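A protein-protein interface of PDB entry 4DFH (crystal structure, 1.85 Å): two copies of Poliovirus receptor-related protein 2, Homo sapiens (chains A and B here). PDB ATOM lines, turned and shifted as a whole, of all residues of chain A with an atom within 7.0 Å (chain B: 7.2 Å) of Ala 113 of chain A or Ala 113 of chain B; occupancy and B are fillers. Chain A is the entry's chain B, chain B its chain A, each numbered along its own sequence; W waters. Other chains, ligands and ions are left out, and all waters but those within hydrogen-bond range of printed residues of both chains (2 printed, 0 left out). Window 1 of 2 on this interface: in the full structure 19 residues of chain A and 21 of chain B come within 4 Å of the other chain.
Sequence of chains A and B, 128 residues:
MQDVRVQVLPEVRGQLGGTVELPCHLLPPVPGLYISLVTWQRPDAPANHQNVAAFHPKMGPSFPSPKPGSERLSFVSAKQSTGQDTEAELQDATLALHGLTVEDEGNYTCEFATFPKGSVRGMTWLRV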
ATOM      1  N   TYR A  34     -25.252  10.312 -10.177  1.00  0.00           N
ATOM      2  CA  TYR A  34     -26.416  11.174 -10.005  1.00  0.00           C
ATOM      3  C   TYR A  34     -26.839  11.861 -11.297  1.00  0.00           C
ATOM      4  O   TYR A  34     -26.010  12.391 -12.031  1.00  0.00           O
ATOM      5  CB  TYR A  34     -26.129  12.225  -8.933  1.00  0.00           C
ATOM      6  CG  TYR A  34     -25.734  11.629  -7.603  1.00  0.00           C
ATOM      7  CD1 TYR A  34     -26.687  11.375  -6.624  1.00  0.00           C
ATOM      8  CD2 TYR A  34     -24.411  11.309  -7.330  1.00  0.00           C
ATOM      9  CE1 TYR A  34     -26.330  10.824  -5.408  1.00  0.00           C
ATOM     10  CE2 TYR A  34     -24.046  10.758  -6.115  1.00  0.00           C
ATOM     11  CZ  TYR A  34     -25.011  10.519  -5.158  1.00  0.00           C
ATOM     12  OH  TYR A  34     -24.655   9.969  -3.947  1.00  0.00           O
ATOM     13  N   ILE A  35     -28.140  11.846 -11.570  1.00  0.00           N
ATOM     14  CA  ILE A  35     -28.687  12.591 -12.697  1.00  0.00           C
ATOM     15  C   ILE A  35     -29.086  13.982 -12.218  1.00  0.00           C
ATOM     16  O   ILE A  35     -30.039  14.138 -11.449  1.00  0.00           O
ATOM     17  CB  ILE A  35     -29.911  11.887 -13.306  1.00  0.00           C
ATOM     18  CG1 ILE A  35     -29.550  10.461 -13.725  1.00  0.00           C
ATOM     19  CG2 ILE A  35     -30.444  12.681 -14.489  1.00  0.00           C
ATOM     20  CD1 ILE A  35     -30.725   9.666 -14.260  1.00  0.00           C
ATOM     21  N   SER A  36     -28.348  14.990 -12.668  1.00  0.00           N
ATOM     22  CA  SER A  36     -28.539  16.354 -12.188  1.00  0.00           C
ATOM     23  C   SER A  36     -29.559  17.112 -13.027  1.00  0.00           C
ATOM     24  O   SER A  36     -30.229  18.021 -12.534  1.00  0.00           O
ATOM     25  CB  SER A  36     -27.207  17.105 -12.184  1.00  0.00           C
ATOM     26  OG  SER A  36     -26.265  16.456 -11.350  1.00  0.00           O
ATOM     27  N   LEU A  37     -29.661  16.740 -14.298  1.00  0.00           N
ATOM     28  CA  LEU A  37     -30.611  17.367 -15.205  1.00  0.00           C
ATOM     29  C   LEU A  37     -30.835  16.493 -16.431  1.00  0.00           C
ATOM     30  O   LEU A  37     -29.933  15.781 -16.874  1.00  0.00           O
ATOM     31  CB  LEU A  37     -30.108  18.747 -15.646  1.00  0.00           C
ATOM     32  CG  LEU A  37     -31.140  19.709 -16.249  1.00  0.00           C
ATOM     33  CD1 LEU A  37     -32.048  20.273 -15.165  1.00  0.00           C
ATOM     34  CD2 LEU A  37     -30.449  20.840 -16.997  1.00  0.00           C
ATOM     35  N   VAL A  38     -32.046  16.552 -16.966  1.00  0.00           N
ATOM     36  CA  VAL A  38     -32.358  15.940 -18.248  1.00  0.00           C
ATOM     37  C   VAL A  38     -32.808  17.032 -19.214  1.00  0.00           C
ATOM     38  O   VAL A  38     -33.570  17.923 -18.837  1.00  0.00           O
ATOM     39  CB  VAL A  38     -33.485  14.905 -18.117  1.00  0.00           C
ATOM     40  CG1 VAL A  38     -34.095  14.611 -19.477  1.00  0.00           C
ATOM     41  CG2 VAL A  38     -32.959  13.633 -17.476  1.00  0.00           C
ATOM     42  N   THR A  39     -32.327  16.978 -20.449  1.00  0.00           N
ATOM     43  CA  THR A  39     -32.765  17.933 -21.463  1.00  0.00           C
ATOM     44  C   THR A  39     -33.042  17.265 -22.802  1.00  0.00           C
ATOM     45  O   THR A  39     -32.430  16.253 -23.147  1.00  0.00           O
ATOM     46  CB  THR A  39     -31.740  19.068 -21.677  1.00  0.00           C
ATOM     47  OG1 THR A  39     -30.543  18.536 -22.256  1.00  0.00           O
ATOM     48  CG2 THR A  39     -31.411  19.752 -20.363  1.00  0.00           C
ATOM     49  N   HIS A  56     -35.714  18.880 -13.973  1.00  0.00           N
ATOM     50  CA  HIS A  56     -34.855  19.008 -12.807  1.00  0.00           C
ATOM     51  C   HIS A  56     -35.389  18.099 -11.704  1.00  0.00           C
ATOM     52  O   HIS A  56     -36.601  17.996 -11.523  1.00  0.00           O
ATOM     53  CB  HIS A  56     -34.837  20.464 -12.340  1.00  0.00           C
ATOM     54  CG  HIS A  56     -33.910  20.720 -11.188  1.00  0.00           C
ATOM     55  ND1 HIS A  56     -32.612  21.137 -11.362  1.00  0.00           N
ATOM     56  CD2 HIS A  56     -34.100  20.613  -9.856  1.00  0.00           C
ATOM     57  CE1 HIS A  56     -32.033  21.279 -10.181  1.00  0.00           C
ATOM     58  NE2 HIS A  56     -32.921  20.965  -9.246  1.00  0.00           N
ATOM     59  N   GLU A 111     -30.424  14.226 -23.523  1.00  0.00           N
ATOM     60  CA  GLU A 111     -29.210  14.355 -22.761  1.00  0.00           C
ATOM     61  C   GLU A 111     -29.377  14.228 -21.241  1.00  0.00           C
ATOM     62  O   GLU A 111     -30.236  14.799 -20.690  1.00  0.00           O
ATOM     63  CB  GLU A 111     -28.540  15.701 -23.029  1.00  0.00           C
ATOM     64  CG  GLU A 111     -27.188  15.795 -22.346  1.00  0.00           C
ATOM     65  CD  GLU A 111     -26.636  17.176 -22.275  1.00  0.00           C
ATOM     66  OE1 GLU A 111     -26.273  17.637 -21.167  1.00  0.00           O
ATOM     67  OE2 GLU A 111     -26.577  17.769 -23.379  1.00  0.00           O
ATOM     68  N   PHE A 112     -28.503  13.446 -20.632  1.00  0.00           N
ATOM     69  CA  PHE A 112     -28.450  13.352 -19.182  1.00  0.00           C
ATOM     70  C   PHE A 112     -27.198  14.074 -18.705  1.00  0.00           C
ATOM     71  O   PHE A 112     -26.085  13.718 -19.097  1.00  0.00           O
ATOM     72  CB  PHE A 112     -28.386  11.890 -18.733  1.00  0.00           C
ATOM     73  CG  PHE A 112     -29.641  11.112 -19.006  1.00  0.00           C
ATOM     74  CD1 PHE A 112     -30.590  10.934 -18.013  1.00  0.00           C
ATOM     75  CD2 PHE A 112     -29.871  10.561 -20.256  1.00  0.00           C
ATOM     76  CE1 PHE A 112     -31.747  10.219 -18.262  1.00  0.00           C
ATOM     77  CE2 PHE A 112     -31.027   9.849 -20.512  1.00  0.00           C
ATOM     78  CZ  PHE A 112     -31.965   9.677 -19.512  1.00  0.00           C
ATOM     79  N   ALA A 113     -27.382  15.097 -17.879  1.00  0.00           N
ATOM     80  CA  ALA A 113     -26.255  15.760 -17.231  1.00  0.00           C
ATOM     81  C   ALA A 113     -26.017  15.065 -15.899  1.00  0.00           C
ATOM     82  O   ALA A 113     -26.770  15.261 -14.948  1.00  0.00           O
ATOM     83  CB  ALA A 113     -26.544  17.241 -17.025  1.00  0.00           C
ATOM     84  N   THR A 114     -24.980  14.233 -15.841  1.00  0.00           N
ATOM     85  CA  THR A 114     -24.751  13.398 -14.667  1.00  0.00           C
ATOM     86  C   THR A 114     -23.479  13.771 -13.920  1.00  0.00           C
ATOM     87  O   THR A 114     -22.568  14.385 -14.476  1.00  0.00           O
ATOM     88  CB  THR A 114     -24.652  11.903 -15.041  1.00  0.00           C
ATOM     89  OG1 THR A 114     -23.354  11.630 -15.583  1.00  0.00           O
ATOM     90  CG2 THR A 114     -25.718  11.524 -16.055  1.00  0.00           C
ATOM     91  N   PHE A 115     -23.427  13.395 -12.650  1.00  0.00           N
ATOM     92  CA  PHE A 115     -22.199  13.495 -11.879  1.00  0.00           C
ATOM     93  C   PHE A 115     -21.951  12.155 -11.201  1.00  0.00           C
ATOM     94  O   PHE A 115     -22.856  11.598 -10.583  1.00  0.00           O
ATOM     95  CB  PHE A 115     -22.279  14.614 -10.841  1.00  0.00           C
ATOM     96  CG  PHE A 115     -20.975  14.876 -10.145  1.00  0.00           C
ATOM     97  CD1 PHE A 115     -20.024  15.703 -10.719  1.00  0.00           C
ATOM     98  CD2 PHE A 115     -20.687  14.273  -8.934  1.00  0.00           C
ATOM     99  CE1 PHE A 115     -18.814  15.937 -10.090  1.00  0.00           C
ATOM    100  CE2 PHE A 115     -19.478  14.504  -8.299  1.00  0.00           C
ATOM    101  CZ  PHE A 115     -18.541  15.334  -8.880  1.00  0.00           C
ATOM    102  N   LYS A 117     -20.046  11.424 -14.019  1.00  0.00           N
ATOM    103  CA  LYS A 117     -19.688  11.014 -15.382  1.00  0.00           C
ATOM    104  C   LYS A 117     -19.817  12.105 -16.450  1.00  0.00           C
ATOM    105  O   LYS A 117     -19.258  11.980 -17.541  1.00  0.00           O
ATOM    106  CB  LYS A 117     -20.484   9.773 -15.797  1.00  0.00           C
ATOM    107  CG  LYS A 117     -20.061   8.496 -15.081  1.00  0.00           C
ATOM    108  CD  LYS A 117     -18.675   8.047 -15.522  1.00  0.00           C
ATOM    109  CE  LYS A 117     -18.255   6.765 -14.811  1.00  0.00           C
ATOM    110  NZ  LYS A 117     -16.931   6.267 -15.290  1.00  0.00           N
ATOM    111  N   GLY A 118     -20.546  13.173 -16.145  1.00  0.00           N
ATOM    112  CA  GLY A 118     -20.717  14.252 -17.102  1.00  0.00           C
ATOM    113  C   GLY A 118     -21.921  14.051 -18.004  1.00  0.00           C
ATOM    114  O   GLY A 118     -22.839  13.302 -17.670  1.00  0.00           O
ATOM    115  N   SER A 119     -21.910  14.714 -19.155  1.00  0.00           N
ATOM    116  CA  SER A 119     -23.057  14.713 -20.060  1.00  0.00           C
ATOM    117  C   SER A 119     -23.014  13.587 -21.094  1.00  0.00           C
ATOM    118  O   SER A 119     -22.010  13.392 -21.777  1.00  0.00           O
ATOM    119  CB  SER A 119     -23.174  16.069 -20.763  1.00  0.00           C
ATOM    120  OG  SER A 119     -24.105  16.013 -21.829  1.00  0.00           O
ATOM    121  N   VAL A 120     -24.147  12.881 -21.237  1.00  0.00           N
ATOM    122  CA  VAL A 120     -24.267  11.779 -22.163  1.00  0.00           C
ATOM    123  C   VAL A 120     -25.563  11.910 -22.966  1.00  0.00           C
ATOM    124  O   VAL A 120     -26.562  12.271 -22.437  1.00  0.00           O
ATOM    125  CB  VAL A 120     -24.146  10.384 -21.491  1.00  0.00           C
ATOM    126  CG1 VAL A 120     -22.820  10.207 -20.895  1.00  0.00           C
ATOM    127  CG2 VAL A 120     -25.148  10.225 -20.472  1.00  0.00           C
ATOM    128  N   TYR B  34     -30.863  28.504 -12.462  1.00  0.00           N
ATOM    129  CA  TYR B  34     -29.974  27.675 -11.659  1.00  0.00           C
ATOM    130  C   TYR B  34     -28.994  26.907 -12.531  1.00  0.00           C
ATOM    131  O   TYR B  34     -29.366  26.379 -13.581  1.00  0.00           O
ATOM    132  CB  TYR B  34     -30.782  26.675 -10.833  1.00  0.00           C
ATOM    133  CG  TYR B  34     -31.813  27.301  -9.924  1.00  0.00           C
ATOM    134  CD1 TYR B  34     -31.544  27.504  -8.576  1.00  0.00           C
ATOM    135  CD2 TYR B  34     -33.057  27.681 -10.411  1.00  0.00           C
ATOM    136  CE1 TYR B  34     -32.484  28.073  -7.741  1.00  0.00           C
ATOM    137  CE2 TYR B  34     -34.003  28.250  -9.581  1.00  0.00           C
ATOM    138  CZ  TYR B  34     -33.710  28.443  -8.249  1.00  0.00           C
ATOM    139  OH  TYR B  34     -34.652  29.009  -7.421  1.00  0.00           O
ATOM    140  N   ILE B  35     -27.741  26.840 -12.088  1.00  0.00           N
ATOM    141  CA  ILE B  35     -26.746  26.007 -12.749  1.00  0.00           C
ATOM    142  C   ILE B  35     -26.703  24.658 -12.046  1.00  0.00           C
ATOM    143  O   ILE B  35     -26.225  24.558 -10.921  1.00  0.00           O
ATOM    144  CB  ILE B  35     -25.344  26.638 -12.705  1.00  0.00           C
ATOM    145  CG1 ILE B  35     -25.349  28.006 -13.393  1.00  0.00           C
ATOM    146  CG2 ILE B  35     -24.327  25.707 -13.362  1.00  0.00           C
ATOM    147  CD1 ILE B  35     -24.088  28.819 -13.148  1.00  0.00           C
ATOM    148  N   SER B  36     -27.214  23.627 -12.710  1.00  0.00           N
ATOM    149  CA  SER B  36     -27.301  22.300 -12.109  1.00  0.00           C
ATOM    150  C   SER B  36     -26.011  21.515 -12.292  1.00  0.00           C
ATOM    151  O   SER B  36     -25.689  20.637 -11.493  1.00  0.00           O
ATOM    152  CB  SER B  36     -28.472  21.519 -12.706  1.00  0.00           C
ATOM    153  OG  SER B  36     -29.704  22.114 -12.346  1.00  0.00           O
ATOM    154  N   LEU B  37     -25.276  21.830 -13.352  1.00  0.00           N
ATOM    155  CA  LEU B  37     -24.022  21.145 -13.629  1.00  0.00           C
ATOM    156  C   LEU B  37     -23.232  21.907 -14.680  1.00  0.00           C
ATOM    157  O   LEU B  37     -23.810  22.574 -15.536  1.00  0.00           O
ATOM    158  CB  LEU B  37     -24.294  19.720 -14.118  1.00  0.00           C
ATOM    159  CG  LEU B  37     -23.116  18.744 -14.137  1.00  0.00           C
ATOM    160  CD1 LEU B  37     -22.832  18.236 -12.733  1.00  0.00           C
ATOM    161  CD2 LEU B  37     -23.404  17.583 -15.077  1.00  0.00           C
ATOM    162  N   VAL B  38     -21.910  21.810 -14.599  1.00  0.00           N
ATOM    163  CA  VAL B  38     -21.026  22.335 -15.632  1.00  0.00           C
ATOM    164  C   VAL B  38     -20.240  21.174 -16.209  1.00  0.00           C
ATOM    165  O   VAL B  38     -19.776  20.312 -15.466  1.00  0.00           O
ATOM    166  CB  VAL B  38     -20.031  23.360 -15.056  1.00  0.00           C
ATOM    167  CG1 VAL B  38     -18.922  23.658 -16.064  1.00  0.00           C
ATOM    168  CG2 VAL B  38     -20.754  24.630 -14.660  1.00  0.00           C
ATOM    169  N   THR B  39     -20.106  21.128 -17.530  1.00  0.00           N
ATOM    170  CA  THR B  39     -19.255  20.118 -18.146  1.00  0.00           C
ATOM    171  C   THR B  39     -18.357  20.720 -19.213  1.00  0.00           C
ATOM    172  O   THR B  39     -18.730  21.676 -19.892  1.00  0.00           O
ATOM    173  CB  THR B  39     -20.056  18.949 -18.771  1.00  0.00           C
ATOM    174  OG1 THR B  39     -20.694  19.381 -19.979  1.00  0.00           O
ATOM    175  CG2 THR B  39     -21.101  18.413 -17.796  1.00  0.00           C
ATOM    176  N   HIS B  56     -20.221  19.854 -10.054  1.00  0.00           N
ATOM    177  CA  HIS B  56     -21.530  19.804  -9.407  1.00  0.00           C
ATOM    178  C   HIS B  56     -21.568  20.803  -8.245  1.00  0.00           C
ATOM    179  O   HIS B  56     -20.603  20.910  -7.486  1.00  0.00           O
ATOM    180  CB  HIS B  56     -21.792  18.379  -8.898  1.00  0.00           C
ATOM    181  CG  HIS B  56     -23.151  18.184  -8.292  1.00  0.00           C
ATOM    182  ND1 HIS B  56     -24.216  17.686  -9.004  1.00  0.00           N
ATOM    183  CD2 HIS B  56     -23.599  18.413  -7.037  1.00  0.00           C
ATOM    184  CE1 HIS B  56     -25.276  17.623  -8.210  1.00  0.00           C
ATOM    185  NE2 HIS B  56     -24.930  18.060  -7.019  1.00  0.00           N
ATOM    186  N   GLU B 111     -20.176  23.693 -21.204  1.00  0.00           N
ATOM    187  CA  GLU B 111     -21.629  23.609 -21.125  1.00  0.00           C
ATOM    188  C   GLU B 111     -22.167  23.851 -19.724  1.00  0.00           C
ATOM    189  O   GLU B 111     -21.678  23.282 -18.746  1.00  0.00           O
ATOM    190  CB  GLU B 111     -22.119  22.247 -21.620  1.00  0.00           C
ATOM    191  CG  GLU B 111     -23.595  22.004 -21.335  1.00  0.00           C
ATOM    192  CD  GLU B 111     -24.016  20.563 -21.560  1.00  0.00           C
ATOM    193  OE1 GLU B 111     -24.882  20.073 -20.804  1.00  0.00           O
ATOM    194  OE2 GLU B 111     -23.483  19.921 -22.489  1.00  0.00           O
ATOM    195  N   PHE B 112     -23.183  24.701 -19.637  1.00  0.00           N
ATOM    196  CA  PHE B 112     -23.926  24.872 -18.402  1.00  0.00           C
ATOM    197  C   PHE B 112     -25.269  24.177 -18.553  1.00  0.00           C
ATOM    198  O   PHE B 112     -26.068  24.543 -19.413  1.00  0.00           O
ATOM    199  CB  PHE B 112     -24.139  26.354 -18.092  1.00  0.00           C
ATOM    200  CG  PHE B 112     -22.866  27.117 -17.877  1.00  0.00           C
ATOM    201  CD1 PHE B 112     -22.352  27.285 -16.602  1.00  0.00           C
ATOM    202  CD2 PHE B 112     -22.183  27.668 -18.950  1.00  0.00           C
ATOM    203  CE1 PHE B 112     -21.179  27.992 -16.402  1.00  0.00           C
ATOM    204  CE2 PHE B 112     -21.009  28.373 -18.755  1.00  0.00           C
ATOM    205  CZ  PHE B 112     -20.508  28.535 -17.480  1.00  0.00           C
ATOM    206  N   ALA B 113     -25.503  23.157 -17.737  1.00  0.00           N
ATOM    207  CA  ALA B 113     -26.811  22.518 -17.683  1.00  0.00           C
ATOM    208  C   ALA B 113     -27.673  23.308 -16.707  1.00  0.00           C
ATOM    209  O   ALA B 113     -27.520  23.182 -15.495  1.00  0.00           O
ATOM    210  CB  ALA B 113     -26.681  21.072 -17.238  1.00  0.00           C
ATOM    211  N   THR B 114     -28.566  24.136 -17.238  1.00  0.00           N
ATOM    212  CA  THR B 114     -29.324  25.053 -16.398  1.00  0.00           C
ATOM    213  C   THR B 114     -30.815  24.741 -16.367  1.00  0.00           C
ATOM    214  O   THR B 114     -31.349  24.085 -17.261  1.00  0.00           O
ATOM    215  CB  THR B 114     -29.157  26.516 -16.852  1.00  0.00           C
ATOM    216  OG1 THR B 114     -30.021  26.775 -17.965  1.00  0.00           O
ATOM    217  CG2 THR B 114     -27.714  26.796 -17.247  1.00  0.00           C
ATOM    218  N   PHE B 115     -31.477  25.219 -15.321  1.00  0.00           N
ATOM    219  CA  PHE B 115     -32.923  25.143 -15.229  1.00  0.00           C
ATOM    220  C   PHE B 115     -33.463  26.530 -14.896  1.00  0.00           C
ATOM    221  O   PHE B 115     -32.966  27.184 -13.981  1.00  0.00           O
ATOM    222  CB  PHE B 115     -33.343  24.140 -14.157  1.00  0.00           C
ATOM    223  CG  PHE B 115     -34.823  23.902 -14.108  1.00  0.00           C
ATOM    224  CD1 PHE B 115     -35.413  22.958 -14.933  1.00  0.00           C
ATOM    225  CD2 PHE B 115     -35.627  24.628 -13.246  1.00  0.00           C
ATOM    226  CE1 PHE B 115     -36.776  22.741 -14.896  1.00  0.00           C
ATOM    227  CE2 PHE B 115     -36.994  24.414 -13.205  1.00  0.00           C
ATOM    228  CZ  PHE B 115     -37.566  23.470 -14.032  1.00  0.00           C
ATOM    229  N   LYS B 117     -33.782  26.989 -18.299  1.00  0.00           N
ATOM    230  CA  LYS B 117     -33.407  27.255 -19.691  1.00  0.00           C
ATOM    231  C   LYS B 117     -32.810  26.063 -20.447  1.00  0.00           C
ATOM    232  O   LYS B 117     -32.817  26.040 -21.678  1.00  0.00           O
ATOM    233  CB  LYS B 117     -32.463  28.457 -19.779  1.00  0.00           C
ATOM    234  CG  LYS B 117     -33.133  29.782 -19.470  1.00  0.00           C
ATOM    235  CD  LYS B 117     -32.205  30.953 -19.750  1.00  0.00           C
ATOM    236  CE  LYS B 117     -32.879  32.280 -19.428  1.00  0.00           C
ATOM    237  NZ  LYS B 117     -34.070  32.520 -20.286  1.00  0.00           N
ATOM    238  N   GLY B 118     -32.296  25.080 -19.720  1.00  0.00           N
ATOM    239  CA  GLY B 118     -31.676  23.930 -20.353  1.00  0.00           C
ATOM    240  C   GLY B 118     -30.188  24.123 -20.598  1.00  0.00           C
ATOM    241  O   GLY B 118     -29.531  24.917 -19.925  1.00  0.00           O
ATOM    242  N   SER B 119     -29.655  23.391 -21.569  1.00  0.00           N
ATOM    243  CA  SER B 119     -28.220  23.391 -21.827  1.00  0.00           C
ATOM    244  C   SER B 119     -27.776  24.562 -22.703  1.00  0.00           C
ATOM    245  O   SER B 119     -28.333  24.800 -23.775  1.00  0.00           O
ATOM    246  CB  SER B 119     -27.799  22.065 -22.463  1.00  0.00           C
ATOM    247  OG  SER B 119     -26.437  22.095 -22.849  1.00  0.00           O
ATOM    248  N   VAL B 120     -26.770  25.291 -22.231  1.00  0.00           N
ATOM    249  CA  VAL B 120     -26.196  26.399 -22.986  1.00  0.00           C
ATOM    250  C   VAL B 120     -24.682  26.238 -23.036  1.00  0.00           C
ATOM    251  O   VAL B 120     -24.055  25.918 -22.032  1.00  0.00           O
ATOM    252  CB  VAL B 120     -26.569  27.760 -22.377  1.00  0.00           C
ATOM    253  CG1 VAL B 120     -28.080  27.970 -22.433  1.00  0.00           C
ATOM    254  CG2 VAL B 120     -26.070  27.860 -20.950  1.00  0.00           C
HETATM  255  O   HOH W   1     -26.036  20.063 -24.863  1.00  0.00           O
HETATM  256  O   HOH W   2     -23.689  18.162 -24.254  1.00  0.00           O
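OE1 of Glu 111 of chain A sits close to OE1 of Glu 111 of chain B (2.8 Å).
OG of Ser 36 of chain A sits at hydrogen-bond distance from ND1 of His 56 of chain B, 3.3 Å away.
OG of Ser 36 of chain B lies within hydrogen-bond range of ND1 of His 56 of chain A, 3.2 Å away.
O of Phe 115 of chain B is in hydrogen-bond range of N of Tyr 34 of chain B (2.9 Å).
N of Ser 36 of chain A lies within hydrogen-bond range of O of Ala 113 of chain A (2.8 Å).
N of Glu 111 of chain A lies within hydrogen-bond range of O of Thr 39 of chain A (2.9 Å).
The side-chain carboxylate (OE1) of Glu 111 of chain A is in hydrogen-bond range of the side-chain hydroxyl (OG) of Ser 119 of chain A (2.8 Å).
OE1 of Glu 111 of chain B lies close to OG of Ser 119 of chain B, at 3.3 Å.
The backbone carbonyl oxygen of Leu 37 of chain A sits at hydrogen-bond distance from the backbone NH of Ala 113 of chain A.
Ser 36 of chain A touches Ser 36 of chain B.
Ala 113 of chain B touches Leu 37 of chain A.
Leu 37 of chain A touches Thr 114 of chain B.
CD1 of Phe 115 of chain B touches CB of His 56 of chain A, at 3.6 Å.
Leu 37 of chain B touches Ala 113 of chain A.
Ala 113 of chain A touches Ala 113 of chain B.
Leu 37 of chain B touches Thr 114 of chain A.
Phe 115 of chain A touches His 56 of chain B.
Of chain B, only Leu 37 and Ala 113 come within 4 Å of Ala 113 of chain A.
Ala 113 of chain B touches just these residues of chain A: Leu 37 (3.7 Å) and Ala 113 (3.8 Å).
Printed residues of chain A within 4 Å of His 56 of chain B: Ser 36 (3.3 Å) and Phe 115 (3.7 Å).
Of the printed residues of chain B, Glu 111 of chain A touches Glu 111 (2.8 Å).
Of the printed residues of chain A, Thr 114 of chain B touches Leu 37 (3.4 Å).
Val 38 of chain A touches none of the printed residues of chain B.
Ile 35 of chain B touches none of the printed residues of chain A.
The nearest residue of chain B that does not touch Ala 113 of chain A is Glu 111 of chain B (5.0 Å).
The nearest residue of chain A that does not touch Ala 113 of chain B is Glu 111 of chain A (5.2 Å).
Of the 16 printed residues of chain A, 7 touch a printed residue of chain B.
Hydrophobic or aromatic side chains of chain B that line the printed part of chain A: Leu 37, His 56, Ala 113 and Phe 115.
Among the printed residues, 11 pairs touch across the chains.
Leu 37 of chain A touches Ala 113 of chain B, and with the chains exchanged Ala 113 of chain A touches Leu 37 of chain B.
Leu 37 of chain A touches Thr 114 of chain B, and with the chains exchanged Thr 114 of chain A touches Leu 37 of chain B.
His 56 of chain A touches Phe 115 of chain B, and with the chains exchanged Phe 115 of chain A touches His 56 of chain B.
Ala 113 of chain A touches its own counterpart, Ala 113 of chain B.
16 positions are printed for both chains.
Water W2 lies within hydrogen-bond range of the side-chain carboxylate of Glu 111 of chain B (2.5 Å), the side-chain carboxylate of Glu 111 of chain A (3.0 Å) and the side-chain hydroxyl of Ser 119 of chain A (3.3 Å).
Water W1 lies within hydrogen-bond range of the side-chain carboxylate of Glu 111 of chain A, the side-chain hydroxyl of Ser 119 of chain B and the side-chain carboxylate of Glu 111 of chain B.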
